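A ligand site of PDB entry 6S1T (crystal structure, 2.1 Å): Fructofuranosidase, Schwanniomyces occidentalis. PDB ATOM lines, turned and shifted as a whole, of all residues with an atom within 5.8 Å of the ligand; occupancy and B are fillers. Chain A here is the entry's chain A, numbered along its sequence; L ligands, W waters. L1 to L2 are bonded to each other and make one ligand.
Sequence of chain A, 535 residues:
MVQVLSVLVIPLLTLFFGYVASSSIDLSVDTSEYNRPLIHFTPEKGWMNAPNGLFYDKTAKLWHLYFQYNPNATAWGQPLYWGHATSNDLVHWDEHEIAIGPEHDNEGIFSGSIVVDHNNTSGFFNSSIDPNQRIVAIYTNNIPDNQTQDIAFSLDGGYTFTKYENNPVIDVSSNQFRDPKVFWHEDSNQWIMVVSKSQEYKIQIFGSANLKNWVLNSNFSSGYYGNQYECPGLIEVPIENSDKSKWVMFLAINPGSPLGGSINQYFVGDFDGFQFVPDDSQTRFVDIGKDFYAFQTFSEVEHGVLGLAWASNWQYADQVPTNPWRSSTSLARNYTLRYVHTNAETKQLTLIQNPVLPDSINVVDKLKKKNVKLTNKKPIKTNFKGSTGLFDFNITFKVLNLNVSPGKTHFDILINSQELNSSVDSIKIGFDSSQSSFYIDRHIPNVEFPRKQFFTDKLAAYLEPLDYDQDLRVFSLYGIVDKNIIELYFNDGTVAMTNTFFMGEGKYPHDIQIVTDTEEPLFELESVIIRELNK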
ATOM      1  N   ASN A  49     -18.154 -19.023  21.003  1.00  0.00           N
ATOM      2  CA  ASN A  49     -19.179 -18.500  21.947  1.00  0.00           C
ATOM      3  C   ASN A  49     -18.456 -17.596  22.973  1.00  0.00           C
ATOM      4  O   ASN A  49     -17.782 -16.660  22.516  1.00  0.00           O
ATOM      5  CB  ASN A  49     -20.166 -19.573  22.438  1.00  0.00           C
ATOM      6  CG  ASN A  49     -19.612 -20.746  23.211  1.00  0.00           C
ATOM      7  OD1 ASN A  49     -18.957 -21.633  22.643  1.00  0.00           O
ATOM      8  ND2 ASN A  49     -19.973 -20.810  24.493  1.00  0.00           N
ATOM      9  N   ALA A  50     -18.640 -17.816  24.267  1.00  0.00           N
ATOM     10  CA  ALA A  50     -18.282 -16.865  25.350  1.00  0.00           C
ATOM     11  C   ALA A  50     -16.830 -16.406  25.252  1.00  0.00           C
ATOM     12  O   ALA A  50     -15.917 -17.223  25.045  1.00  0.00           O
ATOM     13  CB  ALA A  50     -18.574 -17.483  26.702  1.00  0.00           C
ATOM     14  N   GLN A  68     -14.317 -19.417  23.892  1.00  0.00           N
ATOM     15  CA  GLN A  68     -14.853 -20.769  23.658  1.00  0.00           C
ATOM     16  C   GLN A  68     -14.786 -21.024  22.155  1.00  0.00           C
ATOM     17  O   GLN A  68     -15.383 -20.247  21.391  1.00  0.00           O
ATOM     18  CB  GLN A  68     -16.272 -20.868  24.216  1.00  0.00           C
ATOM     19  CG  GLN A  68     -16.329 -20.643  25.727  1.00  0.00           C
ATOM     20  CD  GLN A  68     -15.692 -21.789  26.453  1.00  0.00           C
ATOM     21  OE1 GLN A  68     -14.538 -21.738  26.879  1.00  0.00           O
ATOM     22  NE2 GLN A  68     -16.448 -22.865  26.576  1.00  0.00           N
ATOM     23  N   TRP A  76     -21.370 -25.563  18.313  1.00  0.00           N
ATOM     24  CA  TRP A  76     -20.754 -25.983  19.596  1.00  0.00           C
ATOM     25  C   TRP A  76     -20.439 -27.469  19.517  1.00  0.00           C
ATOM     26  O   TRP A  76     -21.279 -28.219  19.012  1.00  0.00           O
ATOM     27  CB  TRP A  76     -21.681 -25.663  20.757  1.00  0.00           C
ATOM     28  CG  TRP A  76     -20.999 -25.773  22.075  1.00  0.00           C
ATOM     29  CD1 TRP A  76     -20.368 -24.779  22.765  1.00  0.00           C
ATOM     30  CD2 TRP A  76     -20.882 -26.951  22.889  1.00  0.00           C
ATOM     31  NE1 TRP A  76     -19.874 -25.259  23.941  1.00  0.00           N
ATOM     32  CE2 TRP A  76     -20.172 -26.579  24.044  1.00  0.00           C
ATOM     33  CE3 TRP A  76     -21.302 -28.284  22.749  1.00  0.00           C
ATOM     34  CZ2 TRP A  76     -19.890 -27.496  25.062  1.00  0.00           C
ATOM     35  CZ3 TRP A  76     -21.031 -29.184  23.757  1.00  0.00           C
ATOM     36  CH2 TRP A  76     -20.311 -28.791  24.894  1.00  0.00           C
ATOM     37  N   LEU A  80     -13.532 -28.888  22.996  1.00  0.00           N
ATOM     38  CA  LEU A  80     -13.726 -27.411  23.056  1.00  0.00           C
ATOM     39  C   LEU A  80     -12.487 -26.757  23.681  1.00  0.00           C
ATOM     40  O   LEU A  80     -12.039 -27.214  24.737  1.00  0.00           O
ATOM     41  CB  LEU A  80     -14.971 -27.081  23.861  1.00  0.00           C
ATOM     42  CG  LEU A  80     -15.492 -25.647  23.701  1.00  0.00           C
ATOM     43  CD1 LEU A  80     -16.048 -25.413  22.314  1.00  0.00           C
ATOM     44  CD2 LEU A  80     -16.558 -25.361  24.737  1.00  0.00           C
ATOM     45  N   PHE A 110     -13.995 -24.933  29.391  1.00  0.00           N
ATOM     46  CA  PHE A 110     -15.182 -24.050  29.448  1.00  0.00           C
ATOM     47  C   PHE A 110     -14.708 -22.671  29.904  1.00  0.00           C
ATOM     48  O   PHE A 110     -13.495 -22.472  30.072  1.00  0.00           O
ATOM     49  CB  PHE A 110     -16.258 -24.676  30.332  1.00  0.00           C
ATOM     50  CG  PHE A 110     -17.182 -25.666  29.677  1.00  0.00           C
ATOM     51  CD1 PHE A 110     -16.788 -26.415  28.573  1.00  0.00           C
ATOM     52  CD2 PHE A 110     -18.446 -25.885  30.199  1.00  0.00           C
ATOM     53  CE1 PHE A 110     -17.651 -27.327  27.986  1.00  0.00           C
ATOM     54  CE2 PHE A 110     -19.302 -26.804  29.611  1.00  0.00           C
ATOM     55  CZ  PHE A 110     -18.905 -27.525  28.509  1.00  0.00           C
ATOM     56  N   SER A 111     -15.649 -21.750  30.108  1.00  0.00           N
ATOM     57  CA  SER A 111     -15.337 -20.317  30.355  1.00  0.00           C
ATOM     58  C   SER A 111     -14.467 -20.118  31.600  1.00  0.00           C
ATOM     59  O   SER A 111     -14.419 -20.978  32.497  1.00  0.00           O
ATOM     60  CB  SER A 111     -16.591 -19.496  30.405  1.00  0.00           C
ATOM     61  OG  SER A 111     -17.307 -19.669  29.195  1.00  0.00           O
ATOM     62  N   THR A 140     -13.176 -23.537  33.868  1.00  0.00           N
ATOM     63  CA  THR A 140     -13.968 -24.752  34.181  1.00  0.00           C
ATOM     64  C   THR A 140     -13.467 -25.885  33.280  1.00  0.00           C
ATOM     65  O   THR A 140     -13.447 -25.704  32.060  1.00  0.00           O
ATOM     66  CB  THR A 140     -15.467 -24.504  34.032  1.00  0.00           C
ATOM     67  OG1 THR A 140     -15.820 -23.435  34.920  1.00  0.00           O
ATOM     68  CG2 THR A 140     -16.295 -25.723  34.364  1.00  0.00           C
ATOM     69  N   GLN A 147     -17.925 -30.930  36.370  1.00  0.00           N
ATOM     70  CA  GLN A 147     -17.350 -29.581  36.113  1.00  0.00           C
ATOM     71  C   GLN A 147     -16.562 -29.155  37.354  1.00  0.00           C
ATOM     72  O   GLN A 147     -17.128 -29.213  38.473  1.00  0.00           O
ATOM     73  CB  GLN A 147     -18.444 -28.564  35.760  1.00  0.00           C
ATOM     74  CG  GLN A 147     -19.155 -28.903  34.457  1.00  0.00           C
ATOM     75  CD  GLN A 147     -20.193 -27.900  33.994  1.00  0.00           C
ATOM     76  OE1 GLN A 147     -20.728 -27.111  34.767  1.00  0.00           O
ATOM     77  NE2 GLN A 147     -20.479 -27.922  32.713  1.00  0.00           N
ATOM     78  N   GLN A 176     -22.747 -29.047  37.249  1.00  0.00           N
ATOM     79  CA  GLN A 176     -23.360 -27.713  36.989  1.00  0.00           C
ATOM     80  C   GLN A 176     -22.677 -26.694  37.893  1.00  0.00           C
ATOM     81  O   GLN A 176     -23.271 -26.303  38.905  1.00  0.00           O
ATOM     82  CB  GLN A 176     -24.874 -27.752  37.229  1.00  0.00           C
ATOM     83  CG  GLN A 176     -25.623 -28.680  36.291  1.00  0.00           C
ATOM     84  CD  GLN A 176     -25.684 -28.136  34.887  1.00  0.00           C
ATOM     85  OE1 GLN A 176     -25.546 -26.940  34.641  1.00  0.00           O
ATOM     86  NE2 GLN A 176     -25.934 -29.028  33.941  1.00  0.00           N
ATOM     87  N   ARG A 178     -19.582 -23.756  37.083  1.00  0.00           N
ATOM     88  CA  ARG A 178     -18.708 -23.194  36.019  1.00  0.00           C
ATOM     89  C   ARG A 178     -18.667 -21.670  35.977  1.00  0.00           C
ATOM     90  O   ARG A 178     -19.476 -21.007  36.655  1.00  0.00           O
ATOM     91  CB  ARG A 178     -19.156 -23.694  34.648  1.00  0.00           C
ATOM     92  CG  ARG A 178     -20.626 -23.401  34.333  1.00  0.00           C
ATOM     93  CD  ARG A 178     -21.013 -23.879  32.944  1.00  0.00           C
ATOM     94  NE  ARG A 178     -22.426 -23.681  32.643  1.00  0.00           N
ATOM     95  CZ  ARG A 178     -23.411 -24.450  33.097  1.00  0.00           C
ATOM     96  NH1 ARG A 178     -23.157 -25.474  33.885  1.00  0.00           N
ATOM     97  NH2 ARG A 178     -24.669 -24.174  32.794  1.00  0.00           N
ATOM     98  N   ASP A 179     -17.719 -21.182  35.159  1.00  0.00           N
ATOM     99  CA  ASP A 179     -17.506 -19.780  34.720  1.00  0.00           C
ATOM    100  C   ASP A 179     -16.874 -18.950  35.839  1.00  0.00           C
ATOM    101  O   ASP A 179     -17.462 -17.998  36.363  1.00  0.00           O
ATOM    102  CB  ASP A 179     -18.789 -19.192  34.140  1.00  0.00           C
ATOM    103  CG  ASP A 179     -19.499 -20.101  33.154  1.00  0.00           C
ATOM    104  OD1 ASP A 179     -18.838 -20.996  32.595  1.00  0.00           O
ATOM    105  OD2 ASP A 179     -20.705 -19.904  32.956  1.00  0.00           O
ATOM    106  N   GLN A 228     -30.896 -21.145  34.317  1.00  0.00           N
ATOM    107  CA  GLN A 228     -29.580 -21.351  34.978  1.00  0.00           C
ATOM    108  C   GLN A 228     -28.806 -20.040  35.123  1.00  0.00           C
ATOM    109  O   GLN A 228     -28.971 -19.146  34.276  1.00  0.00           O
ATOM    110  CB  GLN A 228     -28.617 -22.202  34.127  1.00  0.00           C
ATOM    111  CG  GLN A 228     -29.118 -23.567  33.732  1.00  0.00           C
ATOM    112  CD  GLN A 228     -28.263 -24.184  32.647  1.00  0.00           C
ATOM    113  OE1 GLN A 228     -28.214 -23.699  31.511  1.00  0.00           O
ATOM    114  NE2 GLN A 228     -27.585 -25.262  32.997  1.00  0.00           N
ATOM    115  N   GLU A 230     -25.033 -18.306  34.895  1.00  0.00           N
ATOM    116  CA  GLU A 230     -23.773 -18.526  34.129  1.00  0.00           C
ATOM    117  C   GLU A 230     -22.905 -17.264  34.172  1.00  0.00           C
ATOM    118  O   GLU A 230     -23.434 -16.205  34.515  1.00  0.00           O
ATOM    119  CB  GLU A 230     -24.093 -18.888  32.691  1.00  0.00           C
ATOM    120  CG  GLU A 230     -24.556 -20.328  32.531  1.00  0.00           C
ATOM    121  CD  GLU A 230     -25.110 -20.721  31.176  1.00  0.00           C
ATOM    122  OE1 GLU A 230     -25.474 -21.913  31.048  1.00  0.00           O
ATOM    123  OE2 GLU A 230     -25.146 -19.876  30.258  1.00  0.00           O
ATOM    124  N   CYS A 231     -21.625 -17.421  33.843  1.00  0.00           N
ATOM    125  CA  CYS A 231     -20.610 -16.334  33.654  1.00  0.00           C
ATOM    126  C   CYS A 231     -20.867 -15.146  34.584  1.00  0.00           C
ATOM    127  O   CYS A 231     -21.207 -14.056  34.110  1.00  0.00           O
ATOM    128  CB  CYS A 231     -20.615 -15.845  32.207  1.00  0.00           C
ATOM    129  SG  CYS A 231     -20.383 -17.172  31.006  1.00  0.00           S
ATOM    130  N   ASN A 254     -29.376 -18.309  30.883  1.00  0.00           N
ATOM    131  CA  ASN A 254     -29.725 -18.966  29.602  1.00  0.00           C
ATOM    132  C   ASN A 254     -30.141 -20.396  29.865  1.00  0.00           C
ATOM    133  O   ASN A 254     -29.478 -21.064  30.668  1.00  0.00           O
ATOM    134  CB  ASN A 254     -28.554 -19.013  28.627  1.00  0.00           C
ATOM    135  CG  ASN A 254     -28.927 -19.739  27.350  1.00  0.00           C
ATOM    136  OD1 ASN A 254     -29.854 -19.315  26.663  1.00  0.00           O
ATOM    137  ND2 ASN A 254     -28.229 -20.809  27.019  1.00  0.00           N
ATOM    138  N   PRO A 255     -31.218 -20.915  29.233  1.00  0.00           N
ATOM    139  CA  PRO A 255     -32.251 -20.085  28.596  1.00  0.00           C
ATOM    140  C   PRO A 255     -33.170 -19.414  29.644  1.00  0.00           C
ATOM    141  O   PRO A 255     -32.799 -19.359  30.799  1.00  0.00           O
ATOM    142  CB  PRO A 255     -32.991 -21.098  27.712  1.00  0.00           C
ATOM    143  CG  PRO A 255     -32.867 -22.381  28.478  1.00  0.00           C
ATOM    144  CD  PRO A 255     -31.473 -22.348  29.058  1.00  0.00           C
ATOM    145  N   TYR A 293     -24.398 -11.664  25.318  1.00  0.00           N
ATOM    146  CA  TYR A 293     -24.365 -12.718  26.350  1.00  0.00           C
ATOM    147  C   TYR A 293     -22.931 -13.057  26.752  1.00  0.00           C
ATOM    148  O   TYR A 293     -22.013 -12.880  25.940  1.00  0.00           O
ATOM    149  CB  TYR A 293     -25.120 -13.968  25.859  1.00  0.00           C
ATOM    150  CG  TYR A 293     -25.374 -14.979  26.950  1.00  0.00           C
ATOM    151  CD1 TYR A 293     -26.161 -14.637  28.035  1.00  0.00           C
ATOM    152  CD2 TYR A 293     -24.805 -16.241  26.923  1.00  0.00           C
ATOM    153  CE1 TYR A 293     -26.405 -15.536  29.055  1.00  0.00           C
ATOM    154  CE2 TYR A 293     -25.045 -17.161  27.931  1.00  0.00           C
ATOM    155  CZ  TYR A 293     -25.843 -16.789  29.019  1.00  0.00           C
ATOM    156  OH  TYR A 293     -26.093 -17.631  30.052  1.00  0.00           O
ATOM    157  N   ALA A 294     -22.768 -13.551  27.991  1.00  0.00           N
ATOM    158  CA  ALA A 294     -21.485 -14.039  28.559  1.00  0.00           C
ATOM    159  C   ALA A 294     -20.496 -12.874  28.617  1.00  0.00           C
ATOM    160  O   ALA A 294     -19.318 -13.044  28.264  1.00  0.00           O
ATOM    161  CB  ALA A 294     -20.970 -15.217  27.765  1.00  0.00           C
ATOM    162  N   TRP A 310     -20.304 -12.030  23.890  1.00  0.00           N
ATOM    163  CA  TRP A 310     -20.634 -12.841  22.698  1.00  0.00           C
ATOM    164  C   TRP A 310     -21.883 -12.223  22.051  1.00  0.00           C
ATOM    165  O   TRP A 310     -22.892 -12.098  22.754  1.00  0.00           O
ATOM    166  CB  TRP A 310     -20.852 -14.284  23.135  1.00  0.00           C
ATOM    167  CG  TRP A 310     -21.266 -15.229  22.061  1.00  0.00           C
ATOM    168  CD1 TRP A 310     -20.666 -15.440  20.852  1.00  0.00           C
ATOM    169  CD2 TRP A 310     -22.363 -16.146  22.151  1.00  0.00           C
ATOM    170  NE1 TRP A 310     -21.337 -16.415  20.173  1.00  0.00           N
ATOM    171  CE2 TRP A 310     -22.374 -16.879  20.940  1.00  0.00           C
ATOM    172  CE3 TRP A 310     -23.332 -16.421  23.115  1.00  0.00           C
ATOM    173  CZ2 TRP A 310     -23.307 -17.864  20.686  1.00  0.00           C
ATOM    174  CZ3 TRP A 310     -24.264 -17.405  22.851  1.00  0.00           C
ATOM    175  CH2 TRP A 310     -24.244 -18.115  21.653  1.00  0.00           C
ATOM    176  N   TRP A 314     -28.329 -18.026  22.227  1.00  0.00           N
ATOM    177  CA  TRP A 314     -28.256 -19.509  22.174  1.00  0.00           C
ATOM    178  C   TRP A 314     -29.421 -20.095  21.375  1.00  0.00           C
ATOM    179  O   TRP A 314     -29.261 -21.196  20.881  1.00  0.00           O
ATOM    180  CB  TRP A 314     -28.183 -20.167  23.559  1.00  0.00           C
ATOM    181  CG  TRP A 314     -26.760 -20.339  23.963  1.00  0.00           C
ATOM    182  CD1 TRP A 314     -26.063 -19.571  24.848  1.00  0.00           C
ATOM    183  CD2 TRP A 314     -25.811 -21.268  23.397  1.00  0.00           C
ATOM    184  NE1 TRP A 314     -24.758 -19.984  24.900  1.00  0.00           N
ATOM    185  CE2 TRP A 314     -24.572 -21.016  24.021  1.00  0.00           C
ATOM    186  CE3 TRP A 314     -25.893 -22.283  22.435  1.00  0.00           C
ATOM    187  CZ2 TRP A 314     -23.425 -21.751  23.725  1.00  0.00           C
ATOM    188  CZ3 TRP A 314     -24.758 -23.003  22.139  1.00  0.00           C
ATOM    189  CH2 TRP A 314     -23.556 -22.755  22.792  1.00  0.00           C
HETATM  190  C1  LIG L   1     -23.127 -22.572  27.369  1.00  0.00           C
HETATM  191  C2  LIG L   1     -24.643 -22.621  27.558  1.00  0.00           C
HETATM  192  C3  LIG L   1     -24.923 -23.663  28.646  1.00  0.00           C
HETATM  193  C4  LIG L   1     -24.425 -25.041  28.228  1.00  0.00           C
HETATM  194  C5  LIG L   1     -22.962 -24.971  27.859  1.00  0.00           C
HETATM  195  C6  LIG L   1     -22.571 -26.304  27.242  1.00  0.00           C
HETATM  196  O1  LIG L   1     -25.119 -21.338  27.969  1.00  0.00           O
HETATM  197  O2  LIG L   1     -26.311 -23.661  28.951  1.00  0.00           O
HETATM  198  O3  LIG L   1     -24.566 -25.966  29.297  1.00  0.00           O
HETATM  199  O4  LIG L   1     -22.698 -23.876  26.955  1.00  0.00           O
HETATM  200  O5  LIG L   1     -23.212 -26.403  25.958  1.00  0.00           O
HETATM  201  C1  LG2 L   2     -22.220 -19.743  28.446  1.00  0.00           C
HETATM  202  C2  LG2 L   2     -21.585 -21.128  28.592  1.00  0.00           C
HETATM  203  C3  LG2 L   2     -20.775 -21.189  29.876  1.00  0.00           C
HETATM  204  C4  LG2 L   2     -19.831 -22.341  29.584  1.00  0.00           C
HETATM  205  C5  LG2 L   2     -19.531 -22.172  28.098  1.00  0.00           C
HETATM  206  C6  LG2 L   2     -19.371 -23.522  27.395  1.00  0.00           C
HETATM  207  O1  LG2 L   2     -22.791 -19.552  27.166  1.00  0.00           O
HETATM  208  O2  LG2 L   2     -22.566 -22.180  28.623  1.00  0.00           O
HETATM  209  O3  LG2 L   2     -21.612 -21.390  31.019  1.00  0.00           O
HETATM  210  O4  LG2 L   2     -18.626 -22.272  30.334  1.00  0.00           O
HETATM  211  O5  LG2 L   2     -20.618 -21.413  27.544  1.00  0.00           O
HETATM  212  O6  LG2 L   2     -18.954 -23.274  26.057  1.00  0.00           O
HETATM  213  O   HOH W   1     -28.199 -24.948  27.292  1.00  0.00           O
HETATM  214  O   HOH W   2     -21.740 -18.317  25.074  1.00  0.00           O
HETATM  215  O   HOH W   3     -26.544 -26.513  31.084  1.00  0.00           O
HETATM  216  O   HOH W   4     -22.618 -27.137  30.948  1.00  0.00           O
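OD2 of Asp 179 sits at hydrogen-bond distance from O3 of LG2 L2, at 2.6 Å. O4 of LG2 L2 is in hydrogen-bond range of N of Ser 111 (3.0 Å). The side-chain amide oxygen of Gln 228 sits at hydrogen-bond distance from an oxygen (O2) of LIG L1. The guanidinium group (NE) of Arg 178 is in hydrogen-bond range of an oxygen (O3) of LG2 L2 (2.9 Å). O4 of LG2 L2 lies within hydrogen-bond range of OG of Ser 111, at 3.1 Å. The side-chain amide nitrogen (ND2) of Asn 254 sits at hydrogen-bond distance from an oxygen (O1) of LIG L1, at 3.3 Å. NE2 of Gln 68 is in hydrogen-bond range of O6 of LG2 L2 (2.6 Å). O6 of LG2 L2 is in hydrogen-bond range of ND2 of Asn 49. An oxygen (O1) of LIG L1 lies within hydrogen-bond range of the side-chain carboxylate of Glu 230, at 2.7 Å. The indole nitrogen of Trp 314 is in hydrogen-bond range of an oxygen (O1) of LG2 L2, at 3.0 Å. An oxygen (O6) of LG2 L2 is in hydrogen-bond range of the indole nitrogen (NE1) of Trp 76 (3.0 Å).
OD2 of Asp 179 sits at hydrogen-bond distance from N of Cys 231 (2.8 Å). The side-chain amide oxygen (OE1) of Gln 176 lies within hydrogen-bond range of the guanidinium group (NH1) of Arg 178 (2.9 Å). The backbone NH of Phe 110 sits at hydrogen-bond distance from the backbone carbonyl oxygen of Thr 140 (2.8 Å). O of Tyr 293 sits at hydrogen-bond distance from N of Trp 310 (2.8 Å). The side-chain hydroxyl of Tyr 293 lies close to the backbone NH of Asn 254, 3.5 Å away. The side-chain hydroxyl of Tyr 293 lies within hydrogen-bond range of the side-chain carboxylate of Glu 230 (2.4 Å). The side-chain carboxylate (OE1) of Glu 230 lies close to the side-chain amide oxygen (OE1) of Gln 228, 3.3 Å away. The backbone NH (N) of Thr 140 is in hydrogen-bond range of the backbone carbonyl oxygen (O) of Ser 111 (3.2 Å).
Merely in contact with the ligand: Tyr 293 (3.4 Å), Phe 110 (3.4 Å) and Leu 80 (3.4 Å). Hydrophobic or aromatic side chains within 4 Å of the ligand: Trp 76, Leu 80, Phe 110, Tyr 293 and Trp 314. 13 residues have an atom within 4 Å of the ligand: Asn 49, Gln 68, Trp 76, Leu 80, Phe 110, Ser 111, Arg 178, Asp 179, Gln 228, Glu 230, Asn 254, Tyr 293 and Trp 314. The nearest printed residue that does not touch the ligand is Cys 231 (4.1 Å).
Water W3 lies within hydrogen-bond range of NE2 of Gln 228, O3 of LIG L1 and NH2 of Arg 178. Water W4 lies within hydrogen-bond range of O3 of LIG L1, NE2 of Gln 147 and NH1 of Arg 178.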
